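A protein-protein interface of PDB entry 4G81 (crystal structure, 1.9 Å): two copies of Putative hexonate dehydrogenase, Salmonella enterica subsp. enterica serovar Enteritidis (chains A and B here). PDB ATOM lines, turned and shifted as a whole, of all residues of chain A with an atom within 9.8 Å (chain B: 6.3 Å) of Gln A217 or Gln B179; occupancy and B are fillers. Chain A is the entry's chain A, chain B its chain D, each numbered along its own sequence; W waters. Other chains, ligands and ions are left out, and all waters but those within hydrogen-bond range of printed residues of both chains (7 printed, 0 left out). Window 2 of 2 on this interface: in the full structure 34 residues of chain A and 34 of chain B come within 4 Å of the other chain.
The backbone carbonyl oxygen (O) of Pro A215 sits at hydrogen-bond distance from the backbone NH (N) of Gln B179 (3.2 Å).
The backbone NH (N) of Gly A250 is in hydrogen-bond range of the side-chain carboxylate (OD1) of Asp A248. The side-chain hydroxyl (OG) of Ser A216 lies within hydrogen-bond range of the backbone carbonyl oxygen (O) of Gly A249 (2.7 Å). The backbone carbonyl oxygen of Gly A249 is in hydrogen-bond range of the side-chain hydroxyl of Thr A214, at 3.1 Å. The backbone carbonyl oxygen (O) of Glu B176 lies within hydrogen-bond range of the side-chain amide nitrogen (NE2) of Gln B179 (3.4 Å). O of Ile B182 sits at hydrogen-bond distance from ND2 of Asn B241 (3.1 Å).
Among the printed residues, merely in contact across the chains: Pro A215 with Ala B174, Pro A215 with Ala B175, Pro A215 with Ala B178, Ser A216 with Ala B178, Gln A217 with Gln B179, Gly A249 with Asn B241, Gly A250 with Asn B241 and Val A254 with Ala B175.
Of the printed residues of chain B, Pro A215 touches Ala B174, Ala B175, Ala B178 and Gln B179. Printed residues of chain B within 4 Å of Ser A216: Ala B178 (3.7 Å). Of chain B, only Gln B179 (3.7 Å) comes within 4 Å of Gln A217. Trp A219 touches none of the printed residues of chain B. Of the printed residues of chain A, Ala B175 touches Pro A215 and Val A254. Of chain A, only Pro A215 (3.2 Å) and Gln A217 (3.7 Å) come within 4 Å of Gln B179. Phe B180 touches none of the printed residues of chain A. The nearest printed residue of chain B that does not touch Gly A249 is Ala B178 (4.2 Å).
Hydrophobic or aromatic side chains of chain A that line the printed part of chain B: Pro A215 and Val A254. Hydrophobic or aromatic side chains of chain B that line the printed part of chain A: Ala B175 and Ala B178. Among the printed residues, 9 pairs touch across the chains.
No position is printed for both chains.
Water W1 lies within hydrogen-bond range of OD1 of Asp A248 (2.5 Å) and N of Asn B241 (3.1 Å). Water W6 lies within hydrogen-bond range of the side-chain amide oxygen of Asn B181 (2.7 Å) and the guanidinium group of Arg A218 (2.9 Å). Water W7 lies within hydrogen-bond range of the backbone carbonyl oxygen (O) of Ala B178 (2.7 Å), the side-chain hydroxyl (OG) of Ser A216 (3.2 Å) and the side-chain amide nitrogen (ND2) of Asn B241 (3.3 Å). Water W5 lies within hydrogen-bond range of the backbone carbonyl oxygen (O) of Asn B241 (2.7 Å) and the side-chain carboxylate (OD1) of Asp A248 (2.8 Å). Water W2 lies within hydrogen-bond range of O of Ala B175 (2.9 Å), N of Gln B179 (2.9 Å), O of Pro A215 (3.0 Å) and N of Ala B178 (3.5 Å). Water W3 bridges O of Ala B178 (2.9 Å) and O of Ser A216 (3.1 Å).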
ATOM      1  N   TYR A 191       8.466 -10.629 -21.553  1.00  0.00           N
ATOM      2  CA  TYR A 191       8.452  -9.189 -21.785  1.00  0.00           C
ATOM      3  C   TYR A 191       7.679  -8.507 -20.673  1.00  0.00           C
ATOM      4  O   TYR A 191       6.448  -8.639 -20.577  1.00  0.00           O
ATOM      5  CB  TYR A 191       7.904  -8.841 -23.169  1.00  0.00           C
ATOM      6  CG  TYR A 191       8.938  -9.073 -24.253  1.00  0.00           C
ATOM      7  CD1 TYR A 191       9.766  -8.042 -24.687  1.00  0.00           C
ATOM      8  CD2 TYR A 191       9.118 -10.335 -24.801  1.00  0.00           C
ATOM      9  CE1 TYR A 191      10.727  -8.262 -25.662  1.00  0.00           C
ATOM     10  CE2 TYR A 191      10.067 -10.564 -25.773  1.00  0.00           C
ATOM     11  CZ  TYR A 191      10.868  -9.526 -26.202  1.00  0.00           C
ATOM     12  OH  TYR A 191      11.820  -9.759 -27.173  1.00  0.00           O
ATOM     13  N   ASP A 207       4.618  -3.432 -29.435  1.00  0.00           N
ATOM     14  CA  ASP A 207       3.570  -3.804 -28.499  1.00  0.00           C
ATOM     15  C   ASP A 207       2.638  -4.842 -29.128  1.00  0.00           C
ATOM     16  O   ASP A 207       2.284  -5.834 -28.490  1.00  0.00           O
ATOM     17  CB  ASP A 207       2.780  -2.565 -28.067  1.00  0.00           C
ATOM     18  CG  ASP A 207       1.673  -2.896 -27.083  1.00  0.00           C
ATOM     19  OD1 ASP A 207       1.983  -3.350 -25.956  1.00  0.00           O
ATOM     20  OD2 ASP A 207       0.493  -2.690 -27.437  1.00  0.00           O
ATOM     21  N   SER A 208       2.256  -4.620 -30.381  1.00  0.00           N
ATOM     22  CA  SER A 208       1.399  -5.568 -31.095  1.00  0.00           C
ATOM     23  C   SER A 208       2.074  -6.928 -31.238  1.00  0.00           C
ATOM     24  O   SER A 208       1.428  -7.976 -31.138  1.00  0.00           O
ATOM     25  CB  SER A 208       1.032  -5.039 -32.479  1.00  0.00           C
ATOM     26  OG  SER A 208       0.274  -3.851 -32.377  1.00  0.00           O
ATOM     27  N   TRP A 209       3.375  -6.910 -31.477  1.00  0.00           N
ATOM     28  CA  TRP A 209       4.118  -8.153 -31.637  1.00  0.00           C
ATOM     29  C   TRP A 209       4.158  -8.945 -30.327  1.00  0.00           C
ATOM     30  O   TRP A 209       3.979 -10.167 -30.316  1.00  0.00           O
ATOM     31  CB  TRP A 209       5.529  -7.855 -32.135  1.00  0.00           C
ATOM     32  CG  TRP A 209       6.397  -9.083 -32.252  1.00  0.00           C
ATOM     33  CD1 TRP A 209       6.236 -10.120 -33.127  1.00  0.00           C
ATOM     34  CD2 TRP A 209       7.564  -9.386 -31.478  1.00  0.00           C
ATOM     35  NE1 TRP A 209       7.230 -11.052 -32.941  1.00  0.00           N
ATOM     36  CE2 TRP A 209       8.061 -10.626 -31.934  1.00  0.00           C
ATOM     37  CE3 TRP A 209       8.242  -8.730 -30.447  1.00  0.00           C
ATOM     38  CZ2 TRP A 209       9.202 -11.221 -31.394  1.00  0.00           C
ATOM     39  CZ3 TRP A 209       9.371  -9.321 -29.908  1.00  0.00           C
ATOM     40  CH2 TRP A 209       9.842 -10.557 -30.385  1.00  0.00           C
ATOM     41  N   VAL A 210       4.401  -8.253 -29.220  1.00  0.00           N
ATOM     42  CA  VAL A 210       4.398  -8.917 -27.924  1.00  0.00           C
ATOM     43  C   VAL A 210       3.028  -9.551 -27.656  1.00  0.00           C
ATOM     44  O   VAL A 210       2.929 -10.714 -27.267  1.00  0.00           O
ATOM     45  CB  VAL A 210       4.770  -7.945 -26.787  1.00  0.00           C
ATOM     46  CG1 VAL A 210       4.441  -8.552 -25.429  1.00  0.00           C
ATOM     47  CG2 VAL A 210       6.244  -7.558 -26.863  1.00  0.00           C
ATOM     48  N   LYS A 211       1.974  -8.782 -27.889  1.00  0.00           N
ATOM     49  CA  LYS A 211       0.622  -9.246 -27.589  1.00  0.00           C
ATOM     50  C   LYS A 211       0.181 -10.405 -28.480  1.00  0.00           C
ATOM     51  O   LYS A 211      -0.647 -11.223 -28.082  1.00  0.00           O
ATOM     52  CB  LYS A 211      -0.365  -8.081 -27.694  1.00  0.00           C
ATOM     53  CG  LYS A 211      -0.270  -7.110 -26.517  1.00  0.00           C
ATOM     54  CD  LYS A 211      -0.993  -5.801 -26.803  1.00  0.00           C
ATOM     55  CE  LYS A 211      -0.949  -4.895 -25.571  1.00  0.00           C
ATOM     56  NZ  LYS A 211      -1.451  -3.525 -25.862  1.00  0.00           N
ATOM     57  N   SER A 212       0.725 -10.466 -29.689  1.00  0.00           N
ATOM     58  CA  SER A 212       0.397 -11.554 -30.605  1.00  0.00           C
ATOM     59  C   SER A 212       1.319 -12.771 -30.395  1.00  0.00           C
ATOM     60  O   SER A 212       1.040 -13.858 -30.905  1.00  0.00           O
ATOM     61  CB  SER A 212       0.433 -11.062 -32.058  1.00  0.00           C
ATOM     62  OG  SER A 212       1.729 -10.614 -32.407  1.00  0.00           O
ATOM     63  N   SER A 213       2.395 -12.596 -29.621  1.00  0.00           N
ATOM     64  CA  SER A 213       3.365 -13.682 -29.394  1.00  0.00           C
ATOM     65  C   SER A 213       3.175 -14.468 -28.101  1.00  0.00           C
ATOM     66  O   SER A 213       3.668 -15.595 -27.969  1.00  0.00           O
ATOM     67  CB  SER A 213       4.790 -13.148 -29.455  1.00  0.00           C
ATOM     68  OG  SER A 213       5.083 -12.678 -30.757  1.00  0.00           O
ATOM     69  N   THR A 214       2.493 -13.863 -27.133  1.00  0.00           N
ATOM     70  CA  THR A 214       2.180 -14.554 -25.887  1.00  0.00           C
ATOM     71  C   THR A 214       0.671 -14.716 -25.820  1.00  0.00           C
ATOM     72  O   THR A 214      -0.074 -13.774 -26.112  1.00  0.00           O
ATOM     73  CB  THR A 214       2.764 -13.828 -24.646  1.00  0.00           C
ATOM     74  OG1 THR A 214       2.326 -14.484 -23.449  1.00  0.00           O
ATOM     75  CG2 THR A 214       2.336 -12.350 -24.609  1.00  0.00           C
ATOM     76  N   PRO A 215       0.204 -15.932 -25.480  1.00  0.00           N
ATOM     77  CA  PRO A 215      -1.243 -16.179 -25.560  1.00  0.00           C
ATOM     78  C   PRO A 215      -2.021 -15.464 -24.462  1.00  0.00           C
ATOM     79  O   PRO A 215      -3.251 -15.433 -24.501  1.00  0.00           O
ATOM     80  CB  PRO A 215      -1.352 -17.702 -25.409  1.00  0.00           C
ATOM     81  CG  PRO A 215      -0.084 -18.101 -24.662  1.00  0.00           C
ATOM     82  CD  PRO A 215       0.971 -17.158 -25.190  1.00  0.00           C
ATOM     83  N   SER A 216      -1.307 -14.897 -23.497  1.00  0.00           N
ATOM     84  CA  SER A 216      -1.934 -14.049 -22.496  1.00  0.00           C
ATOM     85  C   SER A 216      -2.286 -12.690 -23.075  1.00  0.00           C
ATOM     86  O   SER A 216      -3.022 -11.930 -22.453  1.00  0.00           O
ATOM     87  CB  SER A 216      -1.018 -13.871 -21.283  1.00  0.00           C
ATOM     88  OG  SER A 216      -0.961 -15.063 -20.522  1.00  0.00           O
ATOM     89  N   GLN A 217      -1.741 -12.377 -24.248  1.00  0.00           N
ATOM     90  CA  GLN A 217      -2.090 -11.144 -24.964  1.00  0.00           C
ATOM     91  C   GLN A 217      -1.754  -9.876 -24.180  1.00  0.00           C
ATOM     92  O   GLN A 217      -2.431  -8.854 -24.323  1.00  0.00           O
ATOM     93  CB  GLN A 217      -3.582 -11.147 -25.346  1.00  0.00           C
ATOM     94  CG  GLN A 217      -3.952 -12.276 -26.314  1.00  0.00           C
ATOM     95  CD  GLN A 217      -5.433 -12.317 -26.653  1.00  0.00           C
ATOM     96  OE1 GLN A 217      -6.235 -11.569 -26.096  1.00  0.00           O
ATOM     97  NE2 GLN A 217      -5.801 -13.213 -27.562  1.00  0.00           N
ATOM     98  N   ARG A 218      -0.719  -9.941 -23.347  1.00  0.00           N
ATOM     99  CA  ARG A 218      -0.314  -8.774 -22.569  1.00  0.00           C
ATOM    100  C   ARG A 218       1.133  -8.870 -22.105  1.00  0.00           C
ATOM    101  O   ARG A 218       1.711  -9.964 -22.060  1.00  0.00           O
ATOM    102  CB  ARG A 218      -1.212  -8.619 -21.336  1.00  0.00           C
ATOM    103  CG  ARG A 218      -0.998  -9.716 -20.290  1.00  0.00           C
ATOM    104  CD  ARG A 218      -1.969  -9.532 -19.105  1.00  0.00           C
ATOM    105  NE  ARG A 218      -1.824 -10.543 -18.054  1.00  0.00           N
ATOM    106  CZ  ARG A 218      -0.937 -10.480 -17.061  1.00  0.00           C
ATOM    107  NH1 ARG A 218      -0.070  -9.473 -17.008  1.00  0.00           N
ATOM    108  NH2 ARG A 218      -0.901 -11.434 -16.130  1.00  0.00           N
ATOM    109  N   TRP A 219       1.694  -7.723 -21.724  1.00  0.00           N
ATOM    110  CA  TRP A 219       2.986  -7.676 -21.043  1.00  0.00           C
ATOM    111  C   TRP A 219       2.809  -8.135 -19.601  1.00  0.00           C
ATOM    112  O   TRP A 219       1.714  -8.000 -19.032  1.00  0.00           O
ATOM    113  CB  TRP A 219       3.521  -6.238 -21.027  1.00  0.00           C
ATOM    114  CG  TRP A 219       3.882  -5.683 -22.372  1.00  0.00           C
ATOM    115  CD1 TRP A 219       3.020  -5.324 -23.377  1.00  0.00           C
ATOM    116  CD2 TRP A 219       5.202  -5.387 -22.851  1.00  0.00           C
ATOM    117  NE1 TRP A 219       3.731  -4.838 -24.459  1.00  0.00           N
ATOM    118  CE2 TRP A 219       5.072  -4.863 -24.158  1.00  0.00           C
ATOM    119  CE3 TRP A 219       6.483  -5.505 -22.302  1.00  0.00           C
ATOM    120  CZ2 TRP A 219       6.176  -4.471 -24.925  1.00  0.00           C
ATOM    121  CZ3 TRP A 219       7.584  -5.116 -23.068  1.00  0.00           C
ATOM    122  CH2 TRP A 219       7.418  -4.604 -24.361  1.00  0.00           C
ATOM    123  N   GLY A 220       3.878  -8.663 -19.004  1.00  0.00           N
ATOM    124  CA  GLY A 220       3.910  -8.904 -17.570  1.00  0.00           C
ATOM    125  C   GLY A 220       4.323  -7.637 -16.830  1.00  0.00           C
ATOM    126  O   GLY A 220       4.855  -6.702 -17.451  1.00  0.00           O
ATOM    127  N   ASP A 248       6.355 -15.818 -18.718  1.00  0.00           N
ATOM    128  CA  ASP A 248       6.221 -15.182 -20.033  1.00  0.00           C
ATOM    129  C   ASP A 248       4.790 -15.206 -20.579  1.00  0.00           C
ATOM    130  O   ASP A 248       4.557 -14.899 -21.759  1.00  0.00           O
ATOM    131  CB  ASP A 248       7.209 -15.817 -21.028  1.00  0.00           C
ATOM    132  CG  ASP A 248       6.841 -17.254 -21.413  1.00  0.00           C
ATOM    133  OD1 ASP A 248       5.853 -17.819 -20.882  1.00  0.00           O
ATOM    134  OD2 ASP A 248       7.561 -17.827 -22.259  1.00  0.00           O
ATOM    135  N   GLY A 249       3.832 -15.539 -19.708  1.00  0.00           N
ATOM    136  CA  GLY A 249       2.426 -15.556 -20.085  1.00  0.00           C
ATOM    137  C   GLY A 249       2.081 -16.598 -21.145  1.00  0.00           C
ATOM    138  O   GLY A 249       0.961 -16.609 -21.660  1.00  0.00           O
ATOM    139  N   GLY A 250       3.040 -17.460 -21.479  1.00  0.00           N
ATOM    140  CA  GLY A 250       2.827 -18.539 -22.441  1.00  0.00           C
ATOM    141  C   GLY A 250       3.643 -18.429 -23.713  1.00  0.00           C
ATOM    142  O   GLY A 250       3.489 -19.240 -24.639  1.00  0.00           O
ATOM    143  N   TRP A 251       4.514 -17.425 -23.782  1.00  0.00           N
ATOM    144  CA  TRP A 251       5.245 -17.142 -25.020  1.00  0.00           C
ATOM    145  C   TRP A 251       5.980 -18.363 -25.590  1.00  0.00           C
ATOM    146  O   TRP A 251       5.736 -18.767 -26.728  1.00  0.00           O
ATOM    147  CB  TRP A 251       6.239 -15.995 -24.796  1.00  0.00           C
ATOM    148  CG  TRP A 251       6.924 -15.481 -26.051  1.00  0.00           C
ATOM    149  CD1 TRP A 251       7.645 -16.208 -26.959  1.00  0.00           C
ATOM    150  CD2 TRP A 251       6.987 -14.117 -26.491  1.00  0.00           C
ATOM    151  NE1 TRP A 251       8.126 -15.383 -27.952  1.00  0.00           N
ATOM    152  CE2 TRP A 251       7.741 -14.092 -27.685  1.00  0.00           C
ATOM    153  CE3 TRP A 251       6.482 -12.915 -25.989  1.00  0.00           C
ATOM    154  CZ2 TRP A 251       8.000 -12.910 -28.389  1.00  0.00           C
ATOM    155  CZ3 TRP A 251       6.731 -11.735 -26.697  1.00  0.00           C
ATOM    156  CH2 TRP A 251       7.485 -11.745 -27.881  1.00  0.00           C
ATOM    157  N   VAL A 254       4.059 -21.369 -27.175  1.00  0.00           N
ATOM    158  CA  VAL A 254       3.291 -21.232 -28.412  1.00  0.00           C
ATOM    159  C   VAL A 254       4.166 -21.047 -29.646  1.00  0.00           C
ATOM    160  O   VAL A 254       5.157 -20.305 -29.635  1.00  0.00           O
ATOM    161  CB  VAL A 254       2.237 -20.098 -28.324  1.00  0.00           C
ATOM    162  CG1 VAL A 254       1.413 -20.046 -29.590  1.00  0.00           C
ATOM    163  CG2 VAL A 254       1.329 -20.330 -27.128  1.00  0.00           C
ATOM    164  N   ASN B 136     -15.764 -16.259 -16.435  1.00  0.00           N
ATOM    165  CA  ASN B 136     -14.701 -15.259 -16.511  1.00  0.00           C
ATOM    166  C   ASN B 136     -14.113 -15.080 -15.106  1.00  0.00           C
ATOM    167  O   ASN B 136     -13.811 -13.964 -14.678  1.00  0.00           O
ATOM    168  CB  ASN B 136     -15.205 -13.925 -17.090  1.00  0.00           C
ATOM    169  CG  ASN B 136     -14.091 -13.082 -17.678  1.00  0.00           C
ATOM    170  OD1 ASN B 136     -13.134 -13.610 -18.250  1.00  0.00           O
ATOM    171  ND2 ASN B 136     -14.210 -11.764 -17.547  1.00  0.00           N
ATOM    172  N   ALA B 174      -2.288 -23.606 -22.682  1.00  0.00           N
ATOM    173  CA  ALA B 174      -1.791 -22.236 -22.600  1.00  0.00           C
ATOM    174  C   ALA B 174      -2.213 -21.495 -23.856  1.00  0.00           C
ATOM    175  O   ALA B 174      -2.770 -20.393 -23.798  1.00  0.00           O
ATOM    176  CB  ALA B 174      -0.266 -22.228 -22.471  1.00  0.00           C
ATOM    177  N   ALA B 175      -1.959 -22.108 -25.007  1.00  0.00           N
ATOM    178  CA  ALA B 175      -2.238 -21.448 -26.284  1.00  0.00           C
ATOM    179  C   ALA B 175      -3.710 -21.029 -26.415  1.00  0.00           C
ATOM    180  O   ALA B 175      -4.014 -19.918 -26.866  1.00  0.00           O
ATOM    181  CB  ALA B 175      -1.811 -22.357 -27.460  1.00  0.00           C
ATOM    182  N   GLU B 176      -4.629 -21.899 -26.003  1.00  0.00           N
ATOM    183  CA  GLU B 176      -6.054 -21.646 -26.268  1.00  0.00           C
ATOM    184  C   GLU B 176      -6.762 -20.876 -25.161  1.00  0.00           C
ATOM    185  O   GLU B 176      -7.719 -20.151 -25.425  1.00  0.00           O
ATOM    186  CB  GLU B 176      -6.805 -22.962 -26.573  1.00  0.00           C
ATOM    187  CG  GLU B 176      -6.288 -23.688 -27.830  1.00  0.00           C
ATOM    188  CD  GLU B 176      -7.176 -24.846 -28.295  1.00  0.00           C
ATOM    189  OE1 GLU B 176      -8.244 -25.090 -27.690  1.00  0.00           O
ATOM    190  OE2 GLU B 176      -6.792 -25.519 -29.278  1.00  0.00           O
ATOM    191  N   TRP B 177      -6.293 -21.024 -23.925  1.00  0.00           N
ATOM    192  CA  TRP B 177      -7.040 -20.506 -22.767  1.00  0.00           C
ATOM    193  C   TRP B 177      -6.379 -19.391 -21.945  1.00  0.00           C
ATOM    194  O   TRP B 177      -7.031 -18.788 -21.085  1.00  0.00           O
ATOM    195  CB  TRP B 177      -7.391 -21.657 -21.829  1.00  0.00           C
ATOM    196  CG  TRP B 177      -8.235 -22.703 -22.471  1.00  0.00           C
ATOM    197  CD1 TRP B 177      -9.089 -22.541 -23.515  1.00  0.00           C
ATOM    198  CD2 TRP B 177      -8.285 -24.086 -22.112  1.00  0.00           C
ATOM    199  NE1 TRP B 177      -9.682 -23.747 -23.828  1.00  0.00           N
ATOM    200  CE2 TRP B 177      -9.204 -24.712 -22.978  1.00  0.00           C
ATOM    201  CE3 TRP B 177      -7.644 -24.860 -21.137  1.00  0.00           C
ATOM    202  CZ2 TRP B 177      -9.491 -26.081 -22.909  1.00  0.00           C
ATOM    203  CZ3 TRP B 177      -7.940 -26.219 -21.056  1.00  0.00           C
ATOM    204  CH2 TRP B 177      -8.855 -26.814 -21.936  1.00  0.00           C
ATOM    205  N   ALA B 178      -5.101 -19.113 -22.186  1.00  0.00           N
ATOM    206  CA  ALA B 178      -4.426 -18.024 -21.467  1.00  0.00           C
ATOM    207  C   ALA B 178      -5.166 -16.699 -21.656  1.00  0.00           C
ATOM    208  O   ALA B 178      -5.204 -15.853 -20.751  1.00  0.00           O
ATOM    209  CB  ALA B 178      -2.983 -17.892 -21.920  1.00  0.00           C
ATOM    210  N   GLN B 179      -5.776 -16.523 -22.824  1.00  0.00           N
ATOM    211  CA  GLN B 179      -6.500 -15.288 -23.105  1.00  0.00           C
ATOM    212  C   GLN B 179      -7.711 -15.130 -22.196  1.00  0.00           C
ATOM    213  O   GLN B 179      -8.256 -14.038 -22.075  1.00  0.00           O
ATOM    214  CB  GLN B 179      -6.943 -15.230 -24.569  1.00  0.00           C
ATOM    215  CG  GLN B 179      -8.061 -16.197 -24.931  1.00  0.00           C
ATOM    216  CD  GLN B 179      -8.341 -16.191 -26.425  1.00  0.00           C
ATOM    217  OE1 GLN B 179      -8.901 -15.231 -26.956  1.00  0.00           O
ATOM    218  NE2 GLN B 179      -7.928 -17.249 -27.111  1.00  0.00           N
ATOM    219  N   PHE B 180      -8.136 -16.213 -21.555  1.00  0.00           N
ATOM    220  CA  PHE B 180      -9.256 -16.121 -20.610  1.00  0.00           C
ATOM    221  C   PHE B 180      -8.776 -16.079 -19.168  1.00  0.00           C
ATOM    222  O   PHE B 180      -9.543 -16.371 -18.247  1.00  0.00           O
ATOM    223  CB  PHE B 180     -10.210 -17.295 -20.813  1.00  0.00           C
ATOM    224  CG  PHE B 180     -10.749 -17.389 -22.211  1.00  0.00           C
ATOM    225  CD1 PHE B 180     -11.623 -16.423 -22.698  1.00  0.00           C
ATOM    226  CD2 PHE B 180     -10.384 -18.443 -23.044  1.00  0.00           C
ATOM    227  CE1 PHE B 180     -12.131 -16.499 -24.000  1.00  0.00           C
ATOM    228  CE2 PHE B 180     -10.883 -18.529 -24.344  1.00  0.00           C
ATOM    229  CZ  PHE B 180     -11.755 -17.554 -24.825  1.00  0.00           C
ATOM    230  N   ASN B 181      -7.505 -15.729 -18.977  1.00  0.00           N
ATOM    231  CA  ASN B 181      -6.897 -15.679 -17.643  1.00  0.00           C
ATOM    232  C   ASN B 181      -6.936 -17.048 -16.972  1.00  0.00           C
ATOM    233  O   ASN B 181      -7.160 -17.155 -15.764  1.00  0.00           O
ATOM    234  CB  ASN B 181      -7.558 -14.602 -16.751  1.00  0.00           C
ATOM    235  CG  ASN B 181      -6.694 -14.211 -15.553  1.00  0.00           C
ATOM    236  OD1 ASN B 181      -5.482 -14.417 -15.555  1.00  0.00           O
ATOM    237  ND2 ASN B 181      -7.318 -13.618 -14.536  1.00  0.00           N
ATOM    238  N   ILE B 182      -6.727 -18.096 -17.766  1.00  0.00           N
ATOM    239  CA  ILE B 182      -6.496 -19.424 -17.214  1.00  0.00           C
ATOM    240  C   ILE B 182      -5.019 -19.763 -17.401  1.00  0.00           C
ATOM    241  O   ILE B 182      -4.485 -19.647 -18.502  1.00  0.00           O
ATOM    242  CB  ILE B 182      -7.364 -20.497 -17.911  1.00  0.00           C
ATOM    243  CG1 ILE B 182      -8.848 -20.256 -17.633  1.00  0.00           C
ATOM    244  CG2 ILE B 182      -6.972 -21.896 -17.442  1.00  0.00           C
ATOM    245  CD1 ILE B 182      -9.792 -20.972 -18.595  1.00  0.00           C
ATOM    246  N   ASN B 241       2.565 -19.756 -17.910  1.00  0.00           N
ATOM    247  CA  ASN B 241       1.648 -20.521 -18.733  1.00  0.00           C
ATOM    248  C   ASN B 241       2.407 -21.443 -19.666  1.00  0.00           C
ATOM    249  O   ASN B 241       3.400 -21.041 -20.290  1.00  0.00           O
ATOM    250  CB  ASN B 241       0.746 -19.560 -19.521  1.00  0.00           C
ATOM    251  CG  ASN B 241      -0.727 -19.868 -19.350  1.00  0.00           C
ATOM    252  OD1 ASN B 241      -1.135 -21.029 -19.383  1.00  0.00           O
ATOM    253  ND2 ASN B 241      -1.539 -18.824 -19.179  1.00  0.00           N
HETATM  254  O   HOH W   1       5.356 -18.618 -18.518  1.00  0.00           O
HETATM  255  O   HOH W   2      -5.051 -17.722 -25.345  1.00  0.00           O
HETATM  256  O   HOH W   3      -5.056 -12.957 -20.326  1.00  0.00           O
HETATM  257  O   HOH W   4      -0.301 -16.170 -18.023  1.00  0.00           O
HETATM  258  O   HOH W   5       5.628 -20.508 -21.721  1.00  0.00           O
HETATM  259  O   HOH W   6      -3.006 -13.457 -15.718  1.00  0.00           O
HETATM  260  O   HOH W   7      -3.409 -16.078 -18.770  1.00  0.00           O
